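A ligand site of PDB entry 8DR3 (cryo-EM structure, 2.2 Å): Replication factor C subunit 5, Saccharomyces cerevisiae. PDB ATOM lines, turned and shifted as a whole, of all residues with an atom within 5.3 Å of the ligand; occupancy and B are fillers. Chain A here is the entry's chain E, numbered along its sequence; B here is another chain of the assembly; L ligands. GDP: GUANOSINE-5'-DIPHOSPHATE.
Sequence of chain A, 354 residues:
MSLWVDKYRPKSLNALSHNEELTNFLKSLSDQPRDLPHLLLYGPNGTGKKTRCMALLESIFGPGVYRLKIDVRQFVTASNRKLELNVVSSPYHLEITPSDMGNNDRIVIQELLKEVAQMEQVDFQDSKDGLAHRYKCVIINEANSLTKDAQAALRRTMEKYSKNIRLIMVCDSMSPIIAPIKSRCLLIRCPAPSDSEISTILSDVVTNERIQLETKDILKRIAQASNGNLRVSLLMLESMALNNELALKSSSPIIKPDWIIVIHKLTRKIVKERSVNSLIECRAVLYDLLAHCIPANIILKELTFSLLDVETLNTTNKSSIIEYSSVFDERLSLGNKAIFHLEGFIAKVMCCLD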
ATOM      1  N   VAL A   5     -14.112  13.519  -5.807  1.00  0.00           N
ATOM      2  CA  VAL A   5     -14.503  12.933  -4.524  1.00  0.00           C
ATOM      3  C   VAL A   5     -15.887  13.401  -4.125  1.00  0.00           C
ATOM      4  O   VAL A   5     -16.671  12.658  -3.527  1.00  0.00           O
ATOM      5  CB  VAL A   5     -13.448  13.265  -3.447  1.00  0.00           C
ATOM      6  CG1 VAL A   5     -13.436  14.754  -3.150  1.00  0.00           C
ATOM      7  CG2 VAL A   5     -13.712  12.461  -2.183  1.00  0.00           C
ATOM      8  N   ASP A   6     -16.227  14.651  -4.444  1.00  0.00           N
ATOM      9  CA  ASP A   6     -17.530  15.206  -4.094  1.00  0.00           C
ATOM     10  C   ASP A   6     -18.577  14.977  -5.181  1.00  0.00           C
ATOM     11  O   ASP A   6     -19.741  14.743  -4.861  1.00  0.00           O
ATOM     12  CB  ASP A   6     -17.401  16.714  -3.827  1.00  0.00           C
ATOM     13  CG  ASP A   6     -16.566  17.019  -2.596  1.00  0.00           C
ATOM     14  OD1 ASP A   6     -16.661  16.250  -1.611  1.00  0.00           O
ATOM     15  OD2 ASP A   6     -15.831  18.026  -2.607  1.00  0.00           O
ATOM     16  N   TYR A   8     -19.126  12.500  -7.250  1.00  0.00           N
ATOM     17  CA  TYR A   8     -19.655  11.151  -7.377  1.00  0.00           C
ATOM     18  C   TYR A   8     -19.999  10.511  -6.034  1.00  0.00           C
ATOM     19  O   TYR A   8     -20.067   9.282  -5.931  1.00  0.00           O
ATOM     20  CB  TYR A   8     -18.652  10.266  -8.132  1.00  0.00           C
ATOM     21  CG  TYR A   8     -18.384  10.736  -9.538  1.00  0.00           C
ATOM     22  CD1 TYR A   8     -19.355  10.639 -10.524  1.00  0.00           C
ATOM     23  CD2 TYR A   8     -17.154  11.284  -9.889  1.00  0.00           C
ATOM     24  CE1 TYR A   8     -19.113  11.068 -11.808  1.00  0.00           C
ATOM     25  CE2 TYR A   8     -16.902  11.712 -11.172  1.00  0.00           C
ATOM     26  CZ  TYR A   8     -17.887  11.605 -12.132  1.00  0.00           C
ATOM     27  OH  TYR A   8     -17.635  12.033 -13.416  1.00  0.00           O
ATOM     28  N   ARG A   9     -20.222  11.316  -5.000  1.00  0.00           N
ATOM     29  CA  ARG A   9     -20.576  10.775  -3.703  1.00  0.00           C
ATOM     30  C   ARG A   9     -21.996  10.197  -3.744  1.00  0.00           C
ATOM     31  O   ARG A   9     -22.923  10.901  -4.141  1.00  0.00           O
ATOM     32  CB  ARG A   9     -20.482  11.845  -2.619  1.00  0.00           C
ATOM     33  CG  ARG A   9     -20.914  11.358  -1.245  1.00  0.00           C
ATOM     34  CD  ARG A   9     -20.431  12.280  -0.122  1.00  0.00           C
ATOM     35  NE  ARG A   9     -20.771  13.678  -0.378  1.00  0.00           N
ATOM     36  CZ  ARG A   9     -19.908  14.618  -0.749  1.00  0.00           C
ATOM     37  NH1 ARG A   9     -18.620  14.346  -0.914  1.00  0.00           N
ATOM     38  NH2 ARG A   9     -20.341  15.858  -0.943  1.00  0.00           N
ATOM     39  N   PRO A  10     -22.192   8.936  -3.356  1.00  0.00           N
ATOM     40  CA  PRO A  10     -23.548   8.383  -3.376  1.00  0.00           C
ATOM     41  C   PRO A  10     -24.498   9.165  -2.482  1.00  0.00           C
ATOM     42  O   PRO A  10     -24.112   9.678  -1.427  1.00  0.00           O
ATOM     43  CB  PRO A  10     -23.356   6.955  -2.859  1.00  0.00           C
ATOM     44  CG  PRO A  10     -21.917   6.650  -3.071  1.00  0.00           C
ATOM     45  CD  PRO A  10     -21.195   7.943  -2.928  1.00  0.00           C
ATOM     46  N   ALA A  15     -27.160   3.262  -3.539  1.00  0.00           N
ATOM     47  CA  ALA A  15     -26.010   3.692  -4.315  1.00  0.00           C
ATOM     48  C   ALA A  15     -24.674   3.345  -3.661  1.00  0.00           C
ATOM     49  O   ALA A  15     -23.627   3.541  -4.277  1.00  0.00           O
ATOM     50  CB  ALA A  15     -26.076   5.206  -4.546  1.00  0.00           C
ATOM     51  N   LEU A  16     -24.689   2.851  -2.425  1.00  0.00           N
ATOM     52  CA  LEU A  16     -23.453   2.459  -1.761  1.00  0.00           C
ATOM     53  C   LEU A  16     -22.863   1.223  -2.441  1.00  0.00           C
ATOM     54  O   LEU A  16     -23.581   0.341  -2.913  1.00  0.00           O
ATOM     55  CB  LEU A  16     -23.694   2.183  -0.280  1.00  0.00           C
ATOM     56  CG  LEU A  16     -24.309   3.325   0.521  1.00  0.00           C
ATOM     57  CD1 LEU A  16     -24.687   2.865   1.915  1.00  0.00           C
ATOM     58  CD2 LEU A  16     -23.356   4.510   0.586  1.00  0.00           C
ATOM     59  N   SER A  17     -21.538   1.164  -2.478  1.00  0.00           N
ATOM     60  CA  SER A  17     -20.814   0.104  -3.173  1.00  0.00           C
ATOM     61  C   SER A  17     -20.196  -0.906  -2.217  1.00  0.00           C
ATOM     62  O   SER A  17     -20.434  -2.112  -2.360  1.00  0.00           O
ATOM     63  CB  SER A  17     -19.717   0.710  -4.057  1.00  0.00           C
ATOM     64  OG  SER A  17     -20.070   2.012  -4.487  1.00  0.00           O
ATOM     65  N   HIS A  18     -19.398  -0.466  -1.252  1.00  0.00           N
ATOM     66  CA  HIS A  18     -18.662  -1.365  -0.384  1.00  0.00           C
ATOM     67  C   HIS A  18     -19.427  -1.638   0.910  1.00  0.00           C
ATOM     68  O   HIS A  18     -20.334  -0.887   1.293  1.00  0.00           O
ATOM     69  CB  HIS A  18     -17.276  -0.804  -0.071  1.00  0.00           C
ATOM     70  CG  HIS A  18     -17.302   0.524   0.623  1.00  0.00           C
ATOM     71  ND1 HIS A  18     -17.157   0.657   1.985  1.00  0.00           N
ATOM     72  CD2 HIS A  18     -17.424   1.777   0.129  1.00  0.00           C
ATOM     73  CE1 HIS A  18     -17.205   1.931   2.312  1.00  0.00           C
ATOM     74  NE2 HIS A  18     -17.367   2.635   1.205  1.00  0.00           N
ATOM     75  N   PRO A  44     -12.710   4.054  10.907  1.00  0.00           N
ATOM     76  CA  PRO A  44     -11.529   4.777  10.403  1.00  0.00           C
ATOM     77  C   PRO A  44     -11.921   5.971   9.559  1.00  0.00           C
ATOM     78  O   PRO A  44     -12.968   5.989   8.906  1.00  0.00           O
ATOM     79  CB  PRO A  44     -10.786   3.717   9.579  1.00  0.00           C
ATOM     80  CG  PRO A  44     -11.304   2.403  10.061  1.00  0.00           C
ATOM     81  CD  PRO A  44     -12.710   2.639  10.491  1.00  0.00           C
ATOM     82  N   ASN A  45     -11.054   6.977   9.557  1.00  0.00           N
ATOM     83  CA  ASN A  45     -11.336   8.217   8.847  1.00  0.00           C
ATOM     84  C   ASN A  45     -11.448   7.976   7.346  1.00  0.00           C
ATOM     85  O   ASN A  45     -10.723   7.158   6.776  1.00  0.00           O
ATOM     86  CB  ASN A  45     -10.232   9.244   9.120  1.00  0.00           C
ATOM     87  CG  ASN A  45     -10.185   9.680  10.575  1.00  0.00           C
ATOM     88  OD1 ASN A  45      -9.448   9.110  11.374  1.00  0.00           O
ATOM     89  ND2 ASN A  45     -10.970  10.698  10.914  1.00  0.00           N
ATOM     90  N   GLY A  46     -12.376   8.688   6.710  1.00  0.00           N
ATOM     91  CA  GLY A  46     -12.485   8.672   5.272  1.00  0.00           C
ATOM     92  C   GLY A  46     -13.047   7.403   4.680  1.00  0.00           C
ATOM     93  O   GLY A  46     -12.822   7.130   3.490  1.00  0.00           O
ATOM     94  N   THR A  47     -13.783   6.605   5.460  1.00  0.00           N
ATOM     95  CA  THR A  47     -14.347   5.363   4.956  1.00  0.00           C
ATOM     96  C   THR A  47     -15.741   5.528   4.380  1.00  0.00           C
ATOM     97  O   THR A  47     -16.157   4.704   3.561  1.00  0.00           O
ATOM     98  CB  THR A  47     -14.389   4.313   6.083  1.00  0.00           C
ATOM     99  OG1 THR A  47     -15.126   4.827   7.190  1.00  0.00           O
ATOM    100  CG2 THR A  47     -12.988   3.955   6.522  1.00  0.00           C
ATOM    101  N   GLY A  48     -16.476   6.567   4.780  1.00  0.00           N
ATOM    102  CA  GLY A  48     -17.827   6.778   4.285  1.00  0.00           C
ATOM    103  C   GLY A  48     -18.860   6.871   5.388  1.00  0.00           C
ATOM    104  O   GLY A  48     -20.048   6.605   5.142  1.00  0.00           O
ATOM    105  N   LYS A  49     -18.440   7.234   6.593  1.00  0.00           N
ATOM    106  CA  LYS A  49     -19.366   7.314   7.718  1.00  0.00           C
ATOM    107  C   LYS A  49     -20.402   8.405   7.502  1.00  0.00           C
ATOM    108  O   LYS A  49     -21.614   8.172   7.661  1.00  0.00           O
ATOM    109  CB  LYS A  49     -18.599   7.543   9.016  1.00  0.00           C
ATOM    110  CG  LYS A  49     -17.678   6.389   9.407  1.00  0.00           C
ATOM    111  CD  LYS A  49     -17.075   6.593  10.790  1.00  0.00           C
ATOM    112  CE  LYS A  49     -16.130   7.778  10.833  1.00  0.00           C
ATOM    113  NZ  LYS A  49     -15.041   7.693   9.818  1.00  0.00           N
ATOM    114  N   LYS A  50     -19.963   9.611   7.138  1.00  0.00           N
ATOM    115  CA  LYS A  50     -20.894  10.709   6.897  1.00  0.00           C
ATOM    116  C   LYS A  50     -21.794  10.404   5.711  1.00  0.00           C
ATOM    117  O   LYS A  50     -22.992  10.726   5.736  1.00  0.00           O
ATOM    118  CB  LYS A  50     -20.133  12.015   6.678  1.00  0.00           C
ATOM    119  CG  LYS A  50     -20.976  13.267   6.833  1.00  0.00           C
ATOM    120  CD  LYS A  50     -21.370  13.499   8.289  1.00  0.00           C
ATOM    121  CE  LYS A  50     -22.046  14.850   8.468  1.00  0.00           C
ATOM    122  NZ  LYS A  50     -23.034  15.143   7.403  1.00  0.00           N
ATOM    123  N   THR A  51     -21.241   9.799   4.669  1.00  0.00           N
ATOM    124  CA  THR A  51     -22.064   9.423   3.519  1.00  0.00           C
ATOM    125  C   THR A  51     -23.158   8.448   3.918  1.00  0.00           C
ATOM    126  O   THR A  51     -24.305   8.582   3.508  1.00  0.00           O
ATOM    127  CB  THR A  51     -21.173   8.805   2.423  1.00  0.00           C
ATOM    128  OG1 THR A  51     -20.092   9.692   2.128  1.00  0.00           O
ATOM    129  CG2 THR A  51     -21.978   8.544   1.161  1.00  0.00           C
ATOM    130  N   ARG A  52     -22.813   7.453   4.752  1.00  0.00           N
ATOM    131  CA  ARG A  52     -23.807   6.490   5.192  1.00  0.00           C
ATOM    132  C   ARG A  52     -24.852   7.129   6.088  1.00  0.00           C
ATOM    133  O   ARG A  52     -26.043   6.800   6.012  1.00  0.00           O
ATOM    134  CB  ARG A  52     -23.116   5.323   5.906  1.00  0.00           C
ATOM    135  CG  ARG A  52     -22.870   4.120   5.013  1.00  0.00           C
ATOM    136  CD  ARG A  52     -21.511   3.491   5.254  1.00  0.00           C
ATOM    137  NE  ARG A  52     -21.167   2.549   4.191  1.00  0.00           N
ATOM    138  CZ  ARG A  52     -20.604   2.896   3.040  1.00  0.00           C
ATOM    139  NH1 ARG A  52     -20.305   4.149   2.763  1.00  0.00           N
ATOM    140  NH2 ARG A  52     -20.344   1.949   2.138  1.00  0.00           N
ATOM    141  N   VAL A 170     -20.889  10.705  14.960  1.00  0.00           N
ATOM    142  CA  VAL A 170     -19.904  10.082  14.095  1.00  0.00           C
ATOM    143  C   VAL A 170     -18.529  10.300  14.710  1.00  0.00           C
ATOM    144  O   VAL A 170     -18.191  11.422  15.107  1.00  0.00           O
ATOM    145  CB  VAL A 170     -19.965  10.640  12.667  1.00  0.00           C
ATOM    146  CG1 VAL A 170     -19.067   9.839  11.735  1.00  0.00           C
ATOM    147  CG2 VAL A 170     -21.401  10.648  12.160  1.00  0.00           C
ATOM    148  N   ILE A 201     -14.228   1.498  -7.435  1.00  0.00           N
ATOM    149  CA  ILE A 201     -14.726   2.880  -7.382  1.00  0.00           C
ATOM    150  C   ILE A 201     -13.843   3.794  -8.221  1.00  0.00           C
ATOM    151  O   ILE A 201     -14.343   4.634  -8.980  1.00  0.00           O
ATOM    152  CB  ILE A 201     -14.815   3.354  -5.920  1.00  0.00           C
ATOM    153  CG1 ILE A 201     -15.925   2.607  -5.186  1.00  0.00           C
ATOM    154  CG2 ILE A 201     -15.047   4.862  -5.861  1.00  0.00           C
ATOM    155  CD1 ILE A 201     -15.840   2.694  -3.677  1.00  0.00           C
ATOM    156  N   LEU A 230     -10.770   6.077   1.525  1.00  0.00           N
ATOM    157  CA  LEU A 230     -11.361   6.265   0.201  1.00  0.00           C
ATOM    158  C   LEU A 230     -11.260   7.713  -0.254  1.00  0.00           C
ATOM    159  O   LEU A 230     -10.972   7.980  -1.435  1.00  0.00           O
ATOM    160  CB  LEU A 230     -12.826   5.807   0.226  1.00  0.00           C
ATOM    161  CG  LEU A 230     -13.585   5.788  -1.101  1.00  0.00           C
ATOM    162  CD1 LEU A 230     -12.792   5.080  -2.185  1.00  0.00           C
ATOM    163  CD2 LEU A 230     -14.944   5.132  -0.914  1.00  0.00           C
ATOM    164  N   ARG A 231     -11.487   8.668   0.646  1.00  0.00           N
ATOM    165  CA  ARG A 231     -11.379  10.082   0.288  1.00  0.00           C
ATOM    166  C   ARG A 231      -9.964  10.411  -0.173  1.00  0.00           C
ATOM    167  O   ARG A 231      -9.779  11.095  -1.193  1.00  0.00           O
ATOM    168  CB  ARG A 231     -11.775  10.953   1.478  1.00  0.00           C
ATOM    169  CG  ARG A 231     -11.495  12.431   1.294  1.00  0.00           C
ATOM    170  CD  ARG A 231     -12.077  13.264   2.429  1.00  0.00           C
ATOM    171  NE  ARG A 231     -11.523  12.913   3.733  1.00  0.00           N
ATOM    172  CZ  ARG A 231     -12.212  12.432   4.753  1.00  0.00           C
ATOM    173  NH1 ARG A 231     -13.516  12.218   4.676  1.00  0.00           N
ATOM    174  NH2 ARG A 231     -11.583  12.156   5.892  1.00  0.00           N
ATOM    175  N   LEU A 234      -9.413   8.950  -3.698  1.00  0.00           N
ATOM    176  CA  LEU A 234     -10.022   9.726  -4.774  1.00  0.00           C
ATOM    177  C   LEU A 234      -9.271  11.023  -5.020  1.00  0.00           C
ATOM    178  O   LEU A 234      -9.027  11.404  -6.171  1.00  0.00           O
ATOM    179  CB  LEU A 234     -11.485  10.004  -4.445  1.00  0.00           C
ATOM    180  CG  LEU A 234     -12.431   8.812  -4.622  1.00  0.00           C
ATOM    181  CD1 LEU A 234     -13.652   8.960  -3.731  1.00  0.00           C
ATOM    182  CD2 LEU A 234     -12.847   8.659  -6.077  1.00  0.00           C
ATOM    183  N   SER B 695     -17.359  16.831   1.978  1.00  0.00           N
ATOM    184  CA  SER B 695     -17.793  15.887   3.014  1.00  0.00           C
ATOM    185  C   SER B 695     -16.571  15.556   3.867  1.00  0.00           C
ATOM    186  O   SER B 695     -15.840  14.600   3.579  1.00  0.00           O
ATOM    187  CB  SER B 695     -18.413  14.632   2.409  1.00  0.00           C
ATOM    188  OG  SER B 695     -19.013  13.829   3.404  1.00  0.00           O
ATOM    189  N   THR B 696     -16.342  16.337   4.914  1.00  0.00           N
ATOM    190  CA  THR B 696     -15.201  16.141   5.812  1.00  0.00           C
ATOM    191  C   THR B 696     -15.288  17.181   6.923  1.00  0.00           C
ATOM    192  O   THR B 696     -16.129  18.079   6.906  1.00  0.00           O
ATOM    193  CB  THR B 696     -13.872  16.267   5.065  1.00  0.00           C
ATOM    194  OG1 THR B 696     -12.795  16.001   5.968  1.00  0.00           O
ATOM    195  CG2 THR B 696     -13.699  17.655   4.476  1.00  0.00           C
ATOM    196  N   TYR B 705      -8.005  17.770   1.279  1.00  0.00           N
ATOM    197  CA  TYR B 705      -8.570  18.565   0.195  1.00  0.00           C
ATOM    198  C   TYR B 705      -7.596  19.624  -0.305  1.00  0.00           C
ATOM    199  O   TYR B 705      -7.504  19.866  -1.516  1.00  0.00           O
ATOM    200  CB  TYR B 705      -9.876  19.222   0.665  1.00  0.00           C
ATOM    201  CG  TYR B 705     -11.107  18.375   0.472  1.00  0.00           C
ATOM    202  CD1 TYR B 705     -11.827  18.407  -0.707  1.00  0.00           C
ATOM    203  CD2 TYR B 705     -11.552  17.533   1.484  1.00  0.00           C
ATOM    204  CE1 TYR B 705     -12.954  17.639  -0.884  1.00  0.00           C
ATOM    205  CE2 TYR B 705     -12.682  16.757   1.326  1.00  0.00           C
ATOM    206  CZ  TYR B 705     -13.378  16.811   0.137  1.00  0.00           C
ATOM    207  OH  TYR B 705     -14.506  16.038  -0.031  1.00  0.00           O
HETATM  208  PB  GDP L   1     -15.847   9.653   6.770  1.00  0.00           P
HETATM  209  O1B GDP L   1     -15.986   8.216   7.212  1.00  0.00           O
HETATM  210  O2B GDP L   1     -17.078  10.422   7.188  1.00  0.00           O
HETATM  211  O3B GDP L   1     -14.630  10.259   7.406  1.00  0.00           O
HETATM  212  O3A GDP L   1     -15.683   9.712   5.130  1.00  0.00           O
HETATM  213  PA  GDP L   1     -16.860  10.226   4.098  1.00  0.00           P
HETATM  214  O1A GDP L   1     -18.217   9.770   4.580  1.00  0.00           O
HETATM  215  O2A GDP L   1     -16.849  11.731   4.039  1.00  0.00           O
HETATM  216  O5' GDP L   1     -16.560   9.604   2.605  1.00  0.00           O
HETATM  217  C5' GDP L   1     -15.482  10.112   1.874  1.00  0.00           C
HETATM  218  C4' GDP L   1     -15.755  10.000   0.381  1.00  0.00           C
HETATM  219  O4' GDP L   1     -15.704   8.457  -0.060  1.00  0.00           O
HETATM  220  C3' GDP L   1     -16.946  10.450   0.067  1.00  0.00           C
HETATM  221  O3' GDP L   1     -16.860  11.879  -0.365  1.00  0.00           O
HETATM  222  C2' GDP L   1     -17.407   9.572  -1.111  1.00  0.00           C
HETATM  223  O2' GDP L   1     -17.111  10.179  -2.290  1.00  0.00           O
HETATM  224  C1' GDP L   1     -16.606   8.255  -0.983  1.00  0.00           C
HETATM  225  N9  GDP L   1     -17.483   7.143  -0.544  1.00  0.00           N
HETATM  226  C8  GDP L   1     -17.825   6.761   0.690  1.00  0.00           C
HETATM  227  N7  GDP L   1     -18.631   5.693   0.565  1.00  0.00           N
HETATM  228  C5  GDP L   1     -18.773   5.430  -0.731  1.00  0.00           C
HETATM  229  C6  GDP L   1     -19.568   4.336  -1.469  1.00  0.00           C
HETATM  230  O6  GDP L   1     -20.199   3.544  -0.858  1.00  0.00           O
HETATM  231  N1  GDP L   1     -19.540   4.288  -2.901  1.00  0.00           N
HETATM  232  C2  GDP L   1     -18.769   5.249  -3.638  1.00  0.00           C
HETATM  233  N2  GDP L   1     -18.739   5.209  -5.088  1.00  0.00           N
HETATM  234  N3  GDP L   1     -18.023   6.283  -2.922  1.00  0.00           N
HETATM  235  C4  GDP L   1     -18.054   6.339  -1.433  1.00  0.00           C
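O2B of the ligand lies within hydrogen-bond range of N of Lys 50, at 3.0 Å. NZ of Lys 49 is in salt-bridge range of O1B of the ligand (2.8 Å). An oxygen (O1B) of the ligand is in hydrogen-bond range of the side-chain hydroxyl (OG1) of Thr 47 (3.5 Å). The backbone carbonyl oxygen (O) of Ser 695 of chain B sits close to an oxygen (O2A) of the ligand (3.1 Å). The backbone NH (N) of Lys 49 sits at hydrogen-bond distance from an oxygen (O1B) of the ligand, at 2.7 Å. An oxygen (O6) of the ligand sits at hydrogen-bond distance from the backbone NH (N) of Ser 17 (3.2 Å). N of Thr 51 sits at hydrogen-bond distance from O1A of the ligand (3.0 Å). The guanidinium group of Arg 231 lies within salt-bridge range of an oxygen (O2A) of the ligand (3.4 Å). N7 of the ligand is in hydrogen-bond range of NE2 of His 18 (3.4 Å). The side-chain hydroxyl of Ser 17 is in hydrogen-bond range of a nitrogen (N1) of the ligand, at 2.8 Å. OG1 of Thr 51 is in hydrogen-bond range of O1A of the ligand (3.1 Å). The guanidinium group (NH1) of Arg 52 sits at hydrogen-bond distance from a nitrogen (N7) of the ligand, at 3.2 Å. The backbone NH of Thr 47 sits at hydrogen-bond distance from an oxygen (O1B) of the ligand (3.2 Å). An oxygen (O2') of the ligand is in hydrogen-bond range of the backbone carbonyl oxygen of Val 5 (2.8 Å). NH1 of Arg 9 is in hydrogen-bond range of O3' of the ligand (3.1 Å). O2A of the ligand is in hydrogen-bond range of OG of Ser 695 of chain B. The backbone NH of Gly 46 is in hydrogen-bond range of an oxygen (O3B) of the ligand. An oxygen (O1B) of the ligand lies within hydrogen-bond range of the backbone NH (N) of Gly 48 (3.0 Å).
The guanidinium group (NH1) of Arg 9 is in salt-bridge range of the side-chain carboxylate (OD1) of Asp 6 (2.8 Å). The backbone carbonyl oxygen of Gly 48 sits close to the guanidinium group of Arg 52 (3.4 Å). The guanidinium group (NH2) of Arg 52 is in hydrogen-bond range of the backbone carbonyl oxygen (O) of His 18 (3.0 Å). O of Thr 47 sits close to NE2 of His 18. The side-chain amino group of Lys 49 sits at hydrogen-bond distance from the backbone carbonyl oxygen of Pro 44 (2.8 Å). The backbone NH of Leu 230 lies within hydrogen-bond range of the backbone carbonyl oxygen of Gly 46. O of Gly 46 lies within hydrogen-bond range of N of Arg 231 (3.5 Å). The side-chain hydroxyl (OG1) of Thr 47 is in hydrogen-bond range of the backbone carbonyl oxygen (O) of Pro 44, at 3.0 Å.
Residues that only touch the ligand: Leu 230, Pro 10, Leu 16, Ile 201, Asn 45 and Leu 234. Within 4 Å of the ligand: Val 5, Arg 9, Pro 10, Leu 16, Ser 17, His 18, Asn 45, Gly 46, Thr 47, Gly 48, Lys 49, Lys 50, Thr 51, Arg 52, Ile 201, Leu 230, Arg 231, Leu 234 and Ser 695 of chain B. The nearest printed residue that does not touch the ligand is Pro 44 (4.1 Å).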
